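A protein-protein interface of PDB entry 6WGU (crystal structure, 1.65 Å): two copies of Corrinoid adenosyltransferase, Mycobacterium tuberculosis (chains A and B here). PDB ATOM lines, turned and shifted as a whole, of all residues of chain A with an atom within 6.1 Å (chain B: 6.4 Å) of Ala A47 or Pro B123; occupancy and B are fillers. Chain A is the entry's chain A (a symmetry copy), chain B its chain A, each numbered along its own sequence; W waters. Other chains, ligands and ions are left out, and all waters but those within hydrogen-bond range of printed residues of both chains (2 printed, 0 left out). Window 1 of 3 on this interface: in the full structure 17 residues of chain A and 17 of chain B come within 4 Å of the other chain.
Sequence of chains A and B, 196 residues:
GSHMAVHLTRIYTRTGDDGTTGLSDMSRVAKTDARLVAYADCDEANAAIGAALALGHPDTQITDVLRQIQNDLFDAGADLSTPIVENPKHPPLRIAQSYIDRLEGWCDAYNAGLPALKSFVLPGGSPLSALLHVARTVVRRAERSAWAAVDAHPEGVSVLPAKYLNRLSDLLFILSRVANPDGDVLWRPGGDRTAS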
ATOM      1  N   CYS A  42      24.369  16.255   1.904  1.00  0.00           N
ATOM      2  CA  CYS A  42      24.202  14.985   1.201  1.00  0.00           C
ATOM      3  C   CYS A  42      22.762  14.812   0.741  1.00  0.00           C
ATOM      4  O   CYS A  42      22.511  14.323  -0.365  1.00  0.00           O
ATOM      5  CB  CYS A  42      24.585  13.792   2.086  1.00  0.00           C
ATOM      6  SG  CYS A  42      26.331  13.439   2.261  1.00  0.00           S
ATOM      7  N   ASP A  43      21.801  15.197   1.592  1.00  0.00           N
ATOM      8  CA  ASP A  43      20.389  15.159   1.224  1.00  0.00           C
ATOM      9  C   ASP A  43      20.114  16.101   0.056  1.00  0.00           C
ATOM     10  O   ASP A  43      19.427  15.728  -0.899  1.00  0.00           O
ATOM     11  CB  ASP A  43      19.587  15.516   2.462  1.00  0.00           C
ATOM     12  CG  ASP A  43      18.078  15.338   2.310  1.00  0.00           C
ATOM     13  OD1 ASP A  43      17.617  14.549   1.477  1.00  0.00           O
ATOM     14  OD2 ASP A  43      17.355  15.988   3.108  1.00  0.00           O
ATOM     15  N   GLU A  44      20.691  17.310   0.085  1.00  0.00           N
ATOM     16  CA  GLU A  44      20.495  18.242  -1.026  1.00  0.00           C
ATOM     17  C   GLU A  44      21.063  17.661  -2.318  1.00  0.00           C
ATOM     18  O   GLU A  44      20.446  17.773  -3.386  1.00  0.00           O
ATOM     19  CB  GLU A  44      21.133  19.590  -0.699  1.00  0.00           C
ATOM     20  CG  GLU A  44      20.703  20.685  -1.635  1.00  0.00           C
ATOM     21  CD  GLU A  44      21.150  22.064  -1.200  1.00  0.00           C
ATOM     22  OE1 GLU A  44      21.616  22.277  -0.058  1.00  0.00           O
ATOM     23  OE2 GLU A  44      21.015  22.968  -2.027  1.00  0.00           O
ATOM     24  N   ALA A  45      22.239  17.046  -2.250  1.00  0.00           N
ATOM     25  CA  ALA A  45      22.810  16.411  -3.436  1.00  0.00           C
ATOM     26  C   ALA A  45      21.919  15.265  -3.931  1.00  0.00           C
ATOM     27  O   ALA A  45      21.686  15.092  -5.135  1.00  0.00           O
ATOM     28  CB  ALA A  45      24.212  15.909  -3.104  1.00  0.00           C
ATOM     29  N   ASN A  46      21.397  14.480  -3.004  1.00  0.00           N
ATOM     30  CA  ASN A  46      20.505  13.391  -3.371  1.00  0.00           C
ATOM     31  C   ASN A  46      19.266  13.908  -4.083  1.00  0.00           C
ATOM     32  O   ASN A  46      18.829  13.316  -5.075  1.00  0.00           O
ATOM     33  CB  ASN A  46      20.130  12.619  -2.109  1.00  0.00           C
ATOM     34  CG  ASN A  46      19.833  11.156  -2.364  1.00  0.00           C
ATOM     35  OD1 ASN A  46      19.685  10.705  -3.499  1.00  0.00           O
ATOM     36  ND2 ASN A  46      19.742  10.400  -1.290  1.00  0.00           N
ATOM     37  N   ALA A  47      18.685  15.011  -3.592  1.00  0.00           N
ATOM     38  CA  ALA A  47      17.519  15.590  -4.249  1.00  0.00           C
ATOM     39  C   ALA A  47      17.873  16.065  -5.655  1.00  0.00           C
ATOM     40  O   ALA A  47      17.052  15.948  -6.578  1.00  0.00           O
ATOM     41  CB  ALA A  47      16.915  16.722  -3.417  1.00  0.00           C
ATOM     42  N   ALA A  48      19.073  16.648  -5.828  1.00  0.00           N
ATOM     43  CA  ALA A  48      19.506  17.054  -7.166  1.00  0.00           C
ATOM     44  C   ALA A  48      19.573  15.863  -8.128  1.00  0.00           C
ATOM     45  O   ALA A  48      19.168  15.976  -9.295  1.00  0.00           O
ATOM     46  CB  ALA A  48      20.862  17.770  -7.095  1.00  0.00           C
ATOM     47  N   ILE A  49      20.092  14.719  -7.667  1.00  0.00           N
ATOM     48  CA  ILE A  49      20.063  13.507  -8.494  1.00  0.00           C
ATOM     49  C   ILE A  49      18.625  13.084  -8.794  1.00  0.00           C
ATOM     50  O   ILE A  49      18.287  12.738  -9.938  1.00  0.00           O
ATOM     51  CB  ILE A  49      20.875  12.380  -7.829  1.00  0.00           C
ATOM     52  CG1 ILE A  49      22.358  12.795  -7.779  1.00  0.00           C
ATOM     53  CG2 ILE A  49      20.746  11.084  -8.635  1.00  0.00           C
ATOM     54  CD1 ILE A  49      23.265  11.832  -7.121  1.00  0.00           C
ATOM     55  N   GLY A  50      17.738  13.168  -7.800  1.00  0.00           N
ATOM     56  CA  GLY A  50      16.338  12.844  -8.039  1.00  0.00           C
ATOM     57  C   GLY A  50      15.694  13.715  -9.100  1.00  0.00           C
ATOM     58  O   GLY A  50      14.855  13.242  -9.869  1.00  0.00           O
ATOM     59  N   ALA A  51      16.076  14.996  -9.153  1.00  0.00           N
ATOM     60  CA  ALA A  51      15.564  15.873 -10.197  1.00  0.00           C
ATOM     61  C   ALA A  51      16.110  15.498 -11.569  1.00  0.00           C
ATOM     62  O   ALA A  51      15.380  15.556 -12.562  1.00  0.00           O
ATOM     63  CB  ALA A  51      15.881  17.327  -9.842  1.00  0.00           C
ATOM     64  N   ALA A  52      17.389  15.129 -11.645  1.00  0.00           N
ATOM     65  CA  ALA A  52      17.953  14.674 -12.915  1.00  0.00           C
ATOM     66  C   ALA A  52      17.203  13.448 -13.421  1.00  0.00           C
ATOM     67  O   ALA A  52      16.883  13.346 -14.610  1.00  0.00           O
ATOM     68  CB  ALA A  52      19.448  14.387 -12.741  1.00  0.00           C
ATOM     69  N   LEU A  53      16.884  12.521 -12.522  1.00  0.00           N
ATOM     70  CA  LEU A  53      16.130  11.337 -12.916  1.00  0.00           C
ATOM     71  C   LEU A  53      14.732  11.709 -13.400  1.00  0.00           C
ATOM     72  O   LEU A  53      14.239  11.151 -14.393  1.00  0.00           O
ATOM     73  CB  LEU A  53      16.060  10.367 -11.736  1.00  0.00           C
ATOM     74  CG  LEU A  53      17.277   9.487 -11.495  1.00  0.00           C
ATOM     75  CD1 LEU A  53      17.278   8.978 -10.065  1.00  0.00           C
ATOM     76  CD2 LEU A  53      17.308   8.322 -12.461  1.00  0.00           C
ATOM     77  N   GLN A  70      21.750   7.281  -5.315  1.00  0.00           N
ATOM     78  CA  GLN A  70      20.834   7.818  -4.314  1.00  0.00           C
ATOM     79  C   GLN A  70      20.821   6.964  -3.058  1.00  0.00           C
ATOM     80  O   GLN A  70      20.724   7.486  -1.941  1.00  0.00           O
ATOM     81  CB  GLN A  70      19.426   7.911  -4.877  1.00  0.00           C
ATOM     82  CG  GLN A  70      19.298   8.980  -5.946  1.00  0.00           C
ATOM     83  CD  GLN A  70      17.854   9.377  -6.127  1.00  0.00           C
ATOM     84  OE1 GLN A  70      17.040   8.629  -6.712  1.00  0.00           O
ATOM     85  NE2 GLN A  70      17.500  10.536  -5.580  1.00  0.00           N
ATOM     86  N   VAL B 121      12.445   7.131   2.602  1.00  0.00           N
ATOM     87  CA  VAL B 121      12.181   7.687   1.285  1.00  0.00           C
ATOM     88  C   VAL B 121      13.457   8.303   0.723  1.00  0.00           C
ATOM     89  O   VAL B 121      14.168   9.034   1.424  1.00  0.00           O
ATOM     90  CB  VAL B 121      11.050   8.732   1.344  1.00  0.00           C
ATOM     91  CG1 VAL B 121      10.853   9.391   0.008  1.00  0.00           C
ATOM     92  CG2 VAL B 121       9.772   8.062   1.827  1.00  0.00           C
ATOM     93  N   LEU B 122      13.739   8.021  -0.553  1.00  0.00           N
ATOM     94  CA  LEU B 122      14.762   8.749  -1.288  1.00  0.00           C
ATOM     95  C   LEU B 122      14.124   9.860  -2.109  1.00  0.00           C
ATOM     96  O   LEU B 122      12.995   9.720  -2.594  1.00  0.00           O
ATOM     97  CB  LEU B 122      15.522   7.806  -2.224  1.00  0.00           C
ATOM     98  CG  LEU B 122      16.216   6.648  -1.541  1.00  0.00           C
ATOM     99  CD1 LEU B 122      16.898   5.726  -2.551  1.00  0.00           C
ATOM    100  CD2 LEU B 122      17.214   7.127  -0.511  1.00  0.00           C
ATOM    101  N   PRO B 123      14.808  10.979  -2.303  1.00  0.00           N
ATOM    102  CA  PRO B 123      14.160  12.115  -2.957  1.00  0.00           C
ATOM    103  C   PRO B 123      14.002  11.860  -4.445  1.00  0.00           C
ATOM    104  O   PRO B 123      14.974  11.569  -5.154  1.00  0.00           O
ATOM    105  CB  PRO B 123      15.110  13.284  -2.680  1.00  0.00           C
ATOM    106  CG  PRO B 123      16.399  12.664  -2.368  1.00  0.00           C
ATOM    107  CD  PRO B 123      16.124  11.325  -1.741  1.00  0.00           C
ATOM    108  N   GLY B 124      12.787  12.008  -4.926  1.00  0.00           N
ATOM    109  CA  GLY B 124      12.542  11.864  -6.342  1.00  0.00           C
ATOM    110  C   GLY B 124      11.189  11.248  -6.605  1.00  0.00           C
ATOM    111  O   GLY B 124      10.349  11.132  -5.714  1.00  0.00           O
ATOM    112  N   GLY B 125      11.005  10.858  -7.858  1.00  0.00           N
ATOM    113  CA  GLY B 125       9.751  10.293  -8.322  1.00  0.00           C
ATOM    114  C   GLY B 125       9.171  11.029  -9.511  1.00  0.00           C
ATOM    115  O   GLY B 125       9.819  11.148 -10.560  1.00  0.00           O
ATOM    116  N   SER B 129       7.194  15.796  -7.416  1.00  0.00           N
ATOM    117  CA  SER B 129       7.756  15.278  -6.173  1.00  0.00           C
ATOM    118  C   SER B 129       9.249  15.556  -6.089  1.00  0.00           C
ATOM    119  O   SER B 129       9.759  15.961  -5.037  1.00  0.00           O
ATOM    120  CB  SER B 129       7.493  13.781  -6.060  1.00  0.00           C
ATOM    121  OG  SER B 129       8.166  13.209  -4.962  1.00  0.00           O
ATOM    122  N   ALA B 130       9.965  15.357  -7.194  1.00  0.00           N
ATOM    123  CA  ALA B 130      11.396  15.604  -7.171  1.00  0.00           C
ATOM    124  C   ALA B 130      11.696  17.064  -6.873  1.00  0.00           C
ATOM    125  O   ALA B 130      12.642  17.375  -6.130  1.00  0.00           O
ATOM    126  CB  ALA B 130      12.019  15.201  -8.500  1.00  0.00           C
ATOM    127  N   HIS B 133      11.142  17.863  -3.315  1.00  0.00           N
ATOM    128  CA  HIS B 133      12.270  17.402  -2.511  1.00  0.00           C
ATOM    129  C   HIS B 133      13.442  18.369  -2.589  1.00  0.00           C
ATOM    130  O   HIS B 133      14.103  18.617  -1.581  1.00  0.00           O
ATOM    131  CB  HIS B 133      12.724  16.005  -2.938  1.00  0.00           C
ATOM    132  CG  HIS B 133      11.956  14.898  -2.289  1.00  0.00           C
ATOM    133  ND1 HIS B 133      12.167  14.537  -0.977  1.00  0.00           N
ATOM    134  CD2 HIS B 133      11.016  14.052  -2.773  1.00  0.00           C
ATOM    135  CE1 HIS B 133      11.341  13.553  -0.665  1.00  0.00           C
ATOM    136  NE2 HIS B 133      10.657  13.220  -1.745  1.00  0.00           N
ATOM    137  N   VAL B 134      13.775  18.869  -3.783  1.00  0.00           N
ATOM    138  CA  VAL B 134      14.801  19.907  -3.870  1.00  0.00           C
ATOM    139  C   VAL B 134      14.430  21.059  -2.937  1.00  0.00           C
ATOM    140  O   VAL B 134      15.253  21.535  -2.143  1.00  0.00           O
ATOM    141  CB  VAL B 134      14.986  20.375  -5.331  1.00  0.00           C
ATOM    142  CG1 VAL B 134      15.904  21.586  -5.404  1.00  0.00           C
ATOM    143  CG2 VAL B 134      15.556  19.260  -6.220  1.00  0.00           C
ATOM    144  N   ALA B 135      13.196  21.561  -3.058  1.00  0.00           N
ATOM    145  CA  ALA B 135      12.789  22.696  -2.233  1.00  0.00           C
ATOM    146  C   ALA B 135      12.925  22.374  -0.749  1.00  0.00           C
ATOM    147  O   ALA B 135      13.384  23.220   0.047  1.00  0.00           O
ATOM    148  CB  ALA B 135      11.352  23.106  -2.562  1.00  0.00           C
ATOM    149  N   ARG B 136      12.556  21.143  -0.372  1.00  0.00           N
ATOM    150  CA  ARG B 136      12.636  20.732   1.018  1.00  0.00           C
ATOM    151  C   ARG B 136      14.056  20.862   1.524  1.00  0.00           C
ATOM    152  O   ARG B 136      14.295  21.376   2.626  1.00  0.00           O
ATOM    153  CB  ARG B 136      12.148  19.298   1.188  1.00  0.00           C
ATOM    154  CG  ARG B 136      12.271  18.751   2.630  1.00  0.00           C
ATOM    155  CD  ARG B 136      11.842  17.284   2.739  1.00  0.00           C
ATOM    156  NE  ARG B 136      12.572  16.433   1.792  1.00  0.00           N
ATOM    157  CZ  ARG B 136      13.837  16.053   1.950  1.00  0.00           C
ATOM    158  NH1 ARG B 136      14.525  16.407   3.031  1.00  0.00           N
ATOM    159  NH2 ARG B 136      14.426  15.328   1.023  1.00  0.00           N
ATOM    160  N   THR B 137      15.023  20.411   0.720  1.00  0.00           N
ATOM    161  CA  THR B 137      16.402  20.468   1.179  1.00  0.00           C
ATOM    162  C   THR B 137      16.922  21.901   1.251  1.00  0.00           C
ATOM    163  O   THR B 137      17.758  22.198   2.108  1.00  0.00           O
ATOM    164  CB  THR B 137      17.348  19.629   0.315  1.00  0.00           C
ATOM    165  OG1 THR B 137      17.447  20.103  -1.038  1.00  0.00           O
ATOM    166  CG2 THR B 137      16.901  18.179   0.293  1.00  0.00           C
ATOM    167  N   VAL B 185      10.100   6.618  -3.960  1.00  0.00           N
ATOM    168  CA  VAL B 185      11.377   5.926  -4.147  1.00  0.00           C
ATOM    169  C   VAL B 185      11.882   5.535  -2.773  1.00  0.00           C
ATOM    170  O   VAL B 185      11.914   6.380  -1.873  1.00  0.00           O
ATOM    171  CB  VAL B 185      12.398   6.826  -4.863  1.00  0.00           C
ATOM    172  CG1 VAL B 185      13.701   6.058  -5.094  1.00  0.00           C
ATOM    173  CG2 VAL B 185      11.830   7.320  -6.193  1.00  0.00           C
HETATM  174  O   HOH W   1      14.438  15.172  -5.970  1.00  0.00           O
HETATM  175  O   HOH W   2      13.455  10.909  -9.391  1.00  0.00           O
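The backbone NH (N) of Leu B122 is in hydrogen-bond range of the backbone carbonyl oxygen (O) of Val B185 (2.8 Å). A ring nitrogen (ND1) of His B133 lies within hydrogen-bond range of the guanidinium group (NH2) of Arg B136 (3.1 Å). The backbone carbonyl oxygen of Val B134 lies within hydrogen-bond range of the side-chain hydroxyl of Thr B137 (2.8 Å). The side-chain amide oxygen (OD1) of Asn A46 lies close to the side-chain amide nitrogen (NE2) of Gln A70 (3.0 Å). NE2 of Gln A70 lies close to N of Gly A50.
Water W2 lies within hydrogen-bond range of the backbone carbonyl oxygen (O) of Gly A50 (2.8 Å) and the backbone NH (N) of Gly B125 (2.9 Å). Water W1 bridges the backbone carbonyl oxygen (O) of Ala A47 (2.8 Å) and the backbone carbonyl oxygen (O) of Ala B130 (2.8 Å).
Of the printed residues of chain B, Ala A47 touches Pro B123, His B133, Val B134 and Thr B137. Pro B123 touches just these residues of chain A: Asn A46 (3.6 Å), Ala A47 (3.5 Å), Gly A50 (3.4 Å) and Gln A70 (2.8 Å). Of the printed residues of chain B, Asp A43 touches Arg B136 (2.9 Å) and Thr B137 (3.6 Å). Of the printed residues of chain A, Ala B130 touches Gly A50 (3.7 Å) and Ala A51 (3.99 Å). Of the printed residues of chain A, Leu B122 touches Gln A70 (3.8 Å). Of the printed residues of chain B, Gly A50 touches Pro B123 and Ala B130. The nearest residue of chain A that does not touch Pro B123 is Asp A43 (4.5 Å).
No position is printed for both chains.
Hydrophobic or aromatic side chains of chain B within 4 Å of the printed part of chain A: Leu B122, Pro B123, Ala B130 and Val B134. Printed residues of chain A that touch a printed residue of chain B: Asp A43, Glu A44, Asn A46, Ala A47, Gly A50, Ala A51 and Gln A70. Hydrophobic or aromatic side chains of chain A within 4 Å of the printed part of chain B: Ala A47.
O of Pro B123 lies within hydrogen-bond range of NE2 of Gln A70, at 2.8 Å. The guanidinium group of Arg B136 is in salt-bridge range of the side-chain carboxylate of Asp A43 (2.9 Å).
Asp A43 touches Thr B137 (OD2 to CG2, 3.6 Å). OG1 of Thr B137 touches CG of Glu A44 (3.4 Å). Pro B123 touches Asn A46 (CG to C, 3.6 Å). Ala A47 touches Pro B123 (N to CG, 3.5 Å). CB of Ala A47 touches O of His B133, at 3.9 Å. Ala A47 touches Val B134. Ala A47 touches Thr B137 (CB to CG2, 3.99 Å). Gly A50 touches Pro B123. Gly A50 touches Ala B130 (O to CB, 3.7 Å). Gln A70 touches Leu B122.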
